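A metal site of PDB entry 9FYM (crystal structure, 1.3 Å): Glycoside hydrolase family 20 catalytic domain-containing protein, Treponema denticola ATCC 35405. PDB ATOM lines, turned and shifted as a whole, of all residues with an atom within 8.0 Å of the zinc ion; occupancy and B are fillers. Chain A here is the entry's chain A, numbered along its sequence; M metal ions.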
ATOM      1  N   GLU A 113       5.135  -0.224 -14.964  1.00  0.00           N
ATOM      2  CA  GLU A 113       5.150  -0.768 -16.313  1.00  0.00           C
ATOM      3  C   GLU A 113       6.532  -1.146 -16.808  1.00  0.00           C
ATOM      4  O   GLU A 113       6.638  -1.738 -17.886  1.00  0.00           O
ATOM      5  CB  GLU A 113       4.535   0.266 -17.276  1.00  0.00           C
ATOM      6  CG  GLU A 113       5.386   1.541 -17.440  1.00  0.00           C
ATOM      7  CD  GLU A 113       5.079   2.680 -16.455  1.00  0.00           C
ATOM      8  OE1 GLU A 113       4.503   2.450 -15.360  1.00  0.00           O
ATOM      9  OE2 GLU A 113       5.460   3.831 -16.793  1.00  0.00           O
ATOM     10  N   LEU A 114       7.597  -0.804 -16.080  1.00  0.00           N
ATOM     11  CA  LEU A 114       8.954  -1.157 -16.504  1.00  0.00           C
ATOM     12  C   LEU A 114       9.424  -2.452 -15.885  1.00  0.00           C
ATOM     13  O   LEU A 114      10.580  -2.871 -16.076  1.00  0.00           O
ATOM     14  CB  LEU A 114       9.888   0.006 -16.134  1.00  0.00           C
ATOM     15  CG  LEU A 114       9.455   1.336 -16.769  1.00  0.00           C
ATOM     16  CD1 LEU A 114      10.590   2.351 -16.544  1.00  0.00           C
ATOM     17  CD2 LEU A 114       9.144   1.231 -18.236  1.00  0.00           C
ATOM     18  N   ASP A 115       8.545  -3.106 -15.119  1.00  0.00           N
ATOM     19  CA  ASP A 115       8.815  -4.394 -14.504  1.00  0.00           C
ATOM     20  C   ASP A 115       8.852  -5.502 -15.552  1.00  0.00           C
ATOM     21  O   ASP A 115       8.111  -5.482 -16.537  1.00  0.00           O
ATOM     22  CB  ASP A 115       7.666  -4.589 -13.513  1.00  0.00           C
ATOM     23  CG  ASP A 115       7.841  -5.740 -12.576  1.00  0.00           C
ATOM     24  OD1 ASP A 115       8.786  -6.549 -12.651  1.00  0.00           O
ATOM     25  OD2 ASP A 115       6.968  -5.755 -11.678  1.00  0.00           O
ATOM     26  N   GLU A 116       9.726  -6.478 -15.327  1.00  0.00           N
ATOM     27  CA  GLU A 116       9.772  -7.608 -16.263  1.00  0.00           C
ATOM     28  C   GLU A 116       8.570  -8.508 -16.099  1.00  0.00           C
ATOM     29  O   GLU A 116       8.155  -9.173 -17.050  1.00  0.00           O
ATOM     30  CB  GLU A 116      11.052  -8.408 -16.069  1.00  0.00           C
ATOM     31  CG  GLU A 116      11.215  -9.674 -16.919  1.00  0.00           C
ATOM     32  CD  GLU A 116      11.198  -9.412 -18.420  1.00  0.00           C
ATOM     33  OE1 GLU A 116      11.247  -8.232 -18.848  1.00  0.00           O
ATOM     34  OE2 GLU A 116      11.319 -10.389 -19.179  1.00  0.00           O
ATOM     35  N   THR A 117       7.978  -8.506 -14.909  1.00  0.00           N
ATOM     36  CA  THR A 117       6.845  -9.383 -14.573  1.00  0.00           C
ATOM     37  C   THR A 117       5.730  -8.558 -13.967  1.00  0.00           C
ATOM     38  O   THR A 117       5.353  -8.727 -12.797  1.00  0.00           O
ATOM     39  CB  THR A 117       7.289 -10.512 -13.658  1.00  0.00           C
ATOM     40  OG1 THR A 117       7.726  -9.979 -12.391  1.00  0.00           O
ATOM     41  CG2 THR A 117       8.403 -11.247 -14.310  1.00  0.00           C
ATOM     42  N   PRO A 118       5.183  -7.626 -14.734  1.00  0.00           N
ATOM     43  CA  PRO A 118       4.093  -6.799 -14.201  1.00  0.00           C
ATOM     44  C   PRO A 118       2.937  -7.723 -13.824  1.00  0.00           C
ATOM     45  O   PRO A 118       2.737  -8.778 -14.435  1.00  0.00           O
ATOM     46  CB  PRO A 118       3.732  -5.875 -15.377  1.00  0.00           C
ATOM     47  CG  PRO A 118       4.111  -6.672 -16.591  1.00  0.00           C
ATOM     48  CD  PRO A 118       5.340  -7.468 -16.192  1.00  0.00           C
ATOM     49  N   SER A 131      13.126  -7.769 -11.281  1.00  0.00           N
ATOM     50  CA  SER A 131      14.002  -7.258 -12.317  1.00  0.00           C
ATOM     51  C   SER A 131      13.278  -6.241 -13.189  1.00  0.00           C
ATOM     52  O   SER A 131      12.055  -6.254 -13.361  1.00  0.00           O
ATOM     53  CB  SER A 131      14.492  -8.393 -13.231  1.00  0.00           C
ATOM     54  OG  SER A 131      15.447  -9.188 -12.569  1.00  0.00           O
ATOM     55  N   LEU A 132      14.063  -5.314 -13.756  1.00  0.00           N
ATOM     56  CA  LEU A 132      13.546  -4.440 -14.801  1.00  0.00           C
ATOM     57  C   LEU A 132      13.453  -5.195 -16.123  1.00  0.00           C
ATOM     58  O   LEU A 132      14.157  -6.170 -16.357  1.00  0.00           O
ATOM     59  CB  LEU A 132      14.487  -3.260 -15.023  1.00  0.00           C
ATOM     60  CG  LEU A 132      14.731  -2.423 -13.765  1.00  0.00           C
ATOM     61  CD1 LEU A 132      15.732  -1.307 -14.118  1.00  0.00           C
ATOM     62  CD2 LEU A 132      13.418  -1.939 -13.276  1.00  0.00           C
ATOM     63  N   CYS A 133      12.595  -4.703 -17.015  1.00  0.00           N
ATOM     64  CA  CYS A 133      12.500  -5.241 -18.372  1.00  0.00           C
ATOM     65  C   CYS A 133      13.680  -4.746 -19.193  1.00  0.00           C
ATOM     66  O   CYS A 133      13.834  -3.539 -19.406  1.00  0.00           O
ATOM     67  CB  CYS A 133      11.210  -4.757 -19.013  1.00  0.00           C
ATOM     68  SG  CYS A 133      11.097  -5.276 -20.789  1.00  0.00           S
ATOM     69  N   SER A 134      14.504  -5.670 -19.676  1.00  0.00           N
ATOM     70  CA  SER A 134      15.723  -5.333 -20.404  1.00  0.00           C
ATOM     71  C   SER A 134      15.462  -4.898 -21.834  1.00  0.00           C
ATOM     72  O   SER A 134      16.413  -4.444 -22.490  1.00  0.00           O
ATOM     73  CB  SER A 134      16.672  -6.533 -20.392  1.00  0.00           C
ATOM     74  OG  SER A 134      16.273  -7.531 -21.357  1.00  0.00           O
ATOM     75  N   SER A 135      14.235  -5.007 -22.320  1.00  0.00           N
ATOM     76  CA  SER A 135      13.886  -4.539 -23.666  1.00  0.00           C
ATOM     77  C   SER A 135      13.183  -3.197 -23.702  1.00  0.00           C
ATOM     78  O   SER A 135      12.842  -2.707 -24.782  1.00  0.00           O
ATOM     79  CB  SER A 135      12.968  -5.538 -24.386  1.00  0.00           C
ATOM     80  OG  SER A 135      13.571  -6.779 -24.560  1.00  0.00           O
ATOM     81  N   ASN A 136      12.868  -2.616 -22.564  1.00  0.00           N
ATOM     82  CA  ASN A 136      12.064  -1.400 -22.548  1.00  0.00           C
ATOM     83  C   ASN A 136      12.945  -0.155 -22.622  1.00  0.00           C
ATOM     84  O   ASN A 136      13.761   0.111 -21.723  1.00  0.00           O
ATOM     85  CB  ASN A 136      11.192  -1.373 -21.281  1.00  0.00           C
ATOM     86  CG  ASN A 136      10.132  -0.316 -21.334  1.00  0.00           C
ATOM     87  OD1 ASN A 136      10.402   0.856 -21.664  1.00  0.00           O
ATOM     88  ND2 ASN A 136       8.911  -0.705 -21.015  1.00  0.00           N
ATOM     89  N   LEU A 168      14.646 -12.783 -13.232  1.00  0.00           N
ATOM     90  CA  LEU A 168      13.485 -12.729 -14.082  1.00  0.00           C
ATOM     91  C   LEU A 168      13.938 -11.984 -15.331  1.00  0.00           C
ATOM     92  O   LEU A 168      14.333 -10.817 -15.257  1.00  0.00           O
ATOM     93  CB  LEU A 168      12.315 -12.041 -13.386  1.00  0.00           C
ATOM     94  CG  LEU A 168      11.930 -12.711 -12.066  1.00  0.00           C
ATOM     95  CD1 LEU A 168      11.031 -11.809 -11.239  1.00  0.00           C
ATOM     96  CD2 LEU A 168      11.233 -14.061 -12.361  1.00  0.00           C
ATOM     97  N   ILE A 169      13.941 -12.678 -16.457  1.00  0.00           N
ATOM     98  CA  ILE A 169      14.419 -12.103 -17.712  1.00  0.00           C
ATOM     99  C   ILE A 169      13.920 -13.018 -18.829  1.00  0.00           C
ATOM    100  O   ILE A 169      14.070 -14.245 -18.748  1.00  0.00           O
ATOM    101  CB  ILE A 169      15.956 -11.956 -17.686  1.00  0.00           C
ATOM    102  CG1 ILE A 169      16.445 -11.393 -19.021  1.00  0.00           C
ATOM    103  CG2 ILE A 169      16.651 -13.265 -17.334  1.00  0.00           C
ATOM    104  CD1 ILE A 169      17.914 -10.934 -19.006  1.00  0.00           C
ATOM    105  N   GLY A 170      13.308 -12.433 -19.842  1.00  0.00           N
ATOM    106  CA  GLY A 170      12.643 -13.224 -20.891  1.00  0.00           C
ATOM    107  C   GLY A 170      11.433 -13.969 -20.360  1.00  0.00           C
ATOM    108  O   GLY A 170      11.231 -15.137 -20.715  1.00  0.00           O
ATOM    109  N   GLU A 171      10.625 -13.322 -19.523  1.00  0.00           N
ATOM    110  CA  GLU A 171       9.536 -14.016 -18.853  1.00  0.00           C
ATOM    111  C   GLU A 171       8.296 -14.077 -19.731  1.00  0.00           C
ATOM    112  O   GLU A 171       8.025 -13.166 -20.522  1.00  0.00           O
ATOM    113  CB  GLU A 171       9.211 -13.319 -17.525  1.00  0.00           C
ATOM    114  CG  GLU A 171      10.365 -13.330 -16.533  1.00  0.00           C
ATOM    115  CD  GLU A 171      10.793 -14.745 -16.154  1.00  0.00           C
ATOM    116  OE1 GLU A 171       9.881 -15.575 -15.880  1.00  0.00           O
ATOM    117  OE2 GLU A 171      12.014 -15.000 -16.088  1.00  0.00           O
ATOM    118  N   ALA A 173       5.421 -13.503 -18.837  1.00  0.00           N
ATOM    119  CA  ALA A 173       4.590 -12.361 -18.512  1.00  0.00           C
ATOM    120  C   ALA A 173       5.004 -11.098 -19.248  1.00  0.00           C
ATOM    121  O   ALA A 173       4.249 -10.116 -19.256  1.00  0.00           O
ATOM    122  CB  ALA A 173       4.618 -12.084 -17.000  1.00  0.00           C
ATOM    123  N   CYS A 174       6.191 -11.065 -19.839  1.00  0.00           N
ATOM    124  CA  CYS A 174       6.632  -9.840 -20.490  1.00  0.00           C
ATOM    125  C   CYS A 174       6.242  -9.853 -21.957  1.00  0.00           C
ATOM    126  O   CYS A 174       6.671 -10.757 -22.674  1.00  0.00           O
ATOM    127  CB  CYS A 174       8.142  -9.667 -20.392  1.00  0.00           C
ATOM    128  SG  CYS A 174       8.530  -8.026 -21.076  1.00  0.00           S
ATOM    129  N   PRO A 175       5.490  -8.870 -22.446  1.00  0.00           N
ATOM    130  CA  PRO A 175       5.155  -8.839 -23.882  1.00  0.00           C
ATOM    131  C   PRO A 175       6.322  -8.456 -24.796  1.00  0.00           C
ATOM    132  O   PRO A 175       6.290  -8.821 -25.978  1.00  0.00           O
ATOM    133  CB  PRO A 175       3.995  -7.835 -23.962  1.00  0.00           C
ATOM    134  CG  PRO A 175       4.228  -6.917 -22.784  1.00  0.00           C
ATOM    135  CD  PRO A 175       4.811  -7.809 -21.687  1.00  0.00           C
ATOM    136  N   LEU A 176       7.351  -7.772 -24.282  1.00  0.00           N
ATOM    137  CA  LEU A 176       8.523  -7.475 -25.086  1.00  0.00           C
ATOM    138  C   LEU A 176       9.504  -8.642 -25.120  1.00  0.00           C
ATOM    139  O   LEU A 176      10.139  -8.897 -26.148  1.00  0.00           O
ATOM    140  CB  LEU A 176       9.270  -6.244 -24.525  1.00  0.00           C
ATOM    141  CG  LEU A 176       8.661  -4.854 -24.719  1.00  0.00           C
ATOM    142  CD1 LEU A 176       7.447  -4.680 -23.835  1.00  0.00           C
ATOM    143  CD2 LEU A 176       9.669  -3.771 -24.397  1.00  0.00           C
ATOM    144  N   CYS A 177       9.678  -9.343 -23.995  1.00  0.00           N
ATOM    145  CA  CYS A 177      10.780 -10.281 -23.859  1.00  0.00           C
ATOM    146  C   CYS A 177      10.356 -11.747 -23.964  1.00  0.00           C
ATOM    147  O   CYS A 177      11.220 -12.618 -23.995  1.00  0.00           O
ATOM    148  CB  CYS A 177      11.463 -10.089 -22.496  1.00  0.00           C
ATOM    149  SG  CYS A 177      12.252  -8.458 -22.256  1.00  0.00           S
ATOM    150  N   ARG A 178       9.068 -12.055 -23.957  1.00  0.00           N
ATOM    151  CA  ARG A 178       8.680 -13.459 -23.831  1.00  0.00           C
ATOM    152  C   ARG A 178       9.176 -14.276 -25.023  1.00  0.00           C
ATOM    153  O   ARG A 178       9.176 -13.802 -26.158  1.00  0.00           O
ATOM    154  CB  ARG A 178       7.165 -13.573 -23.649  1.00  0.00           C
ATOM    155  CG  ARG A 178       6.333 -13.406 -24.909  1.00  0.00           C
ATOM    156  CD  ARG A 178       4.838 -13.786 -24.658  1.00  0.00           C
ATOM    157  NE  ARG A 178       4.189 -12.870 -23.726  1.00  0.00           N
ATOM    158  CZ  ARG A 178       3.115 -12.124 -24.000  1.00  0.00           C
ATOM    159  NH1 ARG A 178       2.521 -12.158 -25.185  1.00  0.00           N
ATOM    160  NH2 ARG A 178       2.634 -11.314 -23.056  1.00  0.00           N
ATOM    161  N   LYS A 180      12.051 -14.827 -26.017  1.00  0.00           N
ATOM    162  CA  LYS A 180      13.365 -14.432 -26.492  1.00  0.00           C
ATOM    163  C   LYS A 180      14.469 -15.114 -25.703  1.00  0.00           C
ATOM    164  O   LYS A 180      14.303 -15.501 -24.540  1.00  0.00           O
ATOM    165  CB  LYS A 180      13.537 -12.912 -26.420  1.00  0.00           C
ATOM    166  CG  LYS A 180      12.722 -12.121 -27.430  1.00  0.00           C
ATOM    167  CD  LYS A 180      13.142 -10.658 -27.371  1.00  0.00           C
ATOM    168  CE  LYS A 180      13.513 -10.089 -28.727  1.00  0.00           C
ATOM    169  NZ  LYS A 180      14.493  -8.945 -28.573  1.00  0.00           N
ATOM    170  N   LEU A 185      19.158 -11.353 -24.438  1.00  0.00           N
ATOM    171  CA  LEU A 185      18.552 -10.262 -23.658  1.00  0.00           C
ATOM    172  C   LEU A 185      19.583  -9.686 -22.668  1.00  0.00           C
ATOM    173  O   LEU A 185      19.754  -8.460 -22.545  1.00  0.00           O
ATOM    174  CB  LEU A 185      17.329 -10.775 -22.909  1.00  0.00           C
ATOM    175  CG  LEU A 185      16.030 -11.064 -23.698  1.00  0.00           C
ATOM    176  CD1 LEU A 185      14.978 -11.764 -22.868  1.00  0.00           C
ATOM    177  CD2 LEU A 185      15.500  -9.782 -24.280  1.00  0.00           C
HETATM  178 ZN    ZN M   1      10.793  -7.593 -20.670  1.00  0.00          ZN
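The backbone NH (N) of Leu 176 sits close to the side-chain sulfur (SG) of Cys 174 (3.4 Å).
The side-chain hydroxyl (OG) of Ser 135 sits close to the side-chain sulfur (SG) of Cys 177 (3.1 Å).
The backbone carbonyl oxygen of Ser 131 lies within hydrogen-bond range of the backbone NH of Glu 116 (3.1 Å).
The side-chain sulfur (SG) of Cys 133 lies close to the backbone NH (N) of Asn 136 (3.7 Å).
O of Cys 174 lies close to NE of Arg 178, at 3.4 Å.
N of Gly 170 sits at hydrogen-bond distance from OE2 of Glu 116 (2.9 Å).
The backbone NH (N) of Glu 171 sits at hydrogen-bond distance from the side-chain carboxylate (OE2) of Glu 116, 3.0 Å away.
N of Ser 135 lies close to SG of Cys 133 (3.5 Å).
Of the 24 residues printed, 4 come within 4 Å of the zinc ion.
The nearest printed residue that does not touch the zinc ion is Ser 134 (4.3 Å).
The zinc ion is bound by the side-chain carboxylate (OE1) of Glu 116 (2.0 Å).
The zinc ion is bound by SG of Cys 177, at 2.3 Å.
The zinc ion is bound by SG of Cys 174, at 2.3 Å.
The zinc ion is bound by SG of Cys 133 (2.3 Å).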
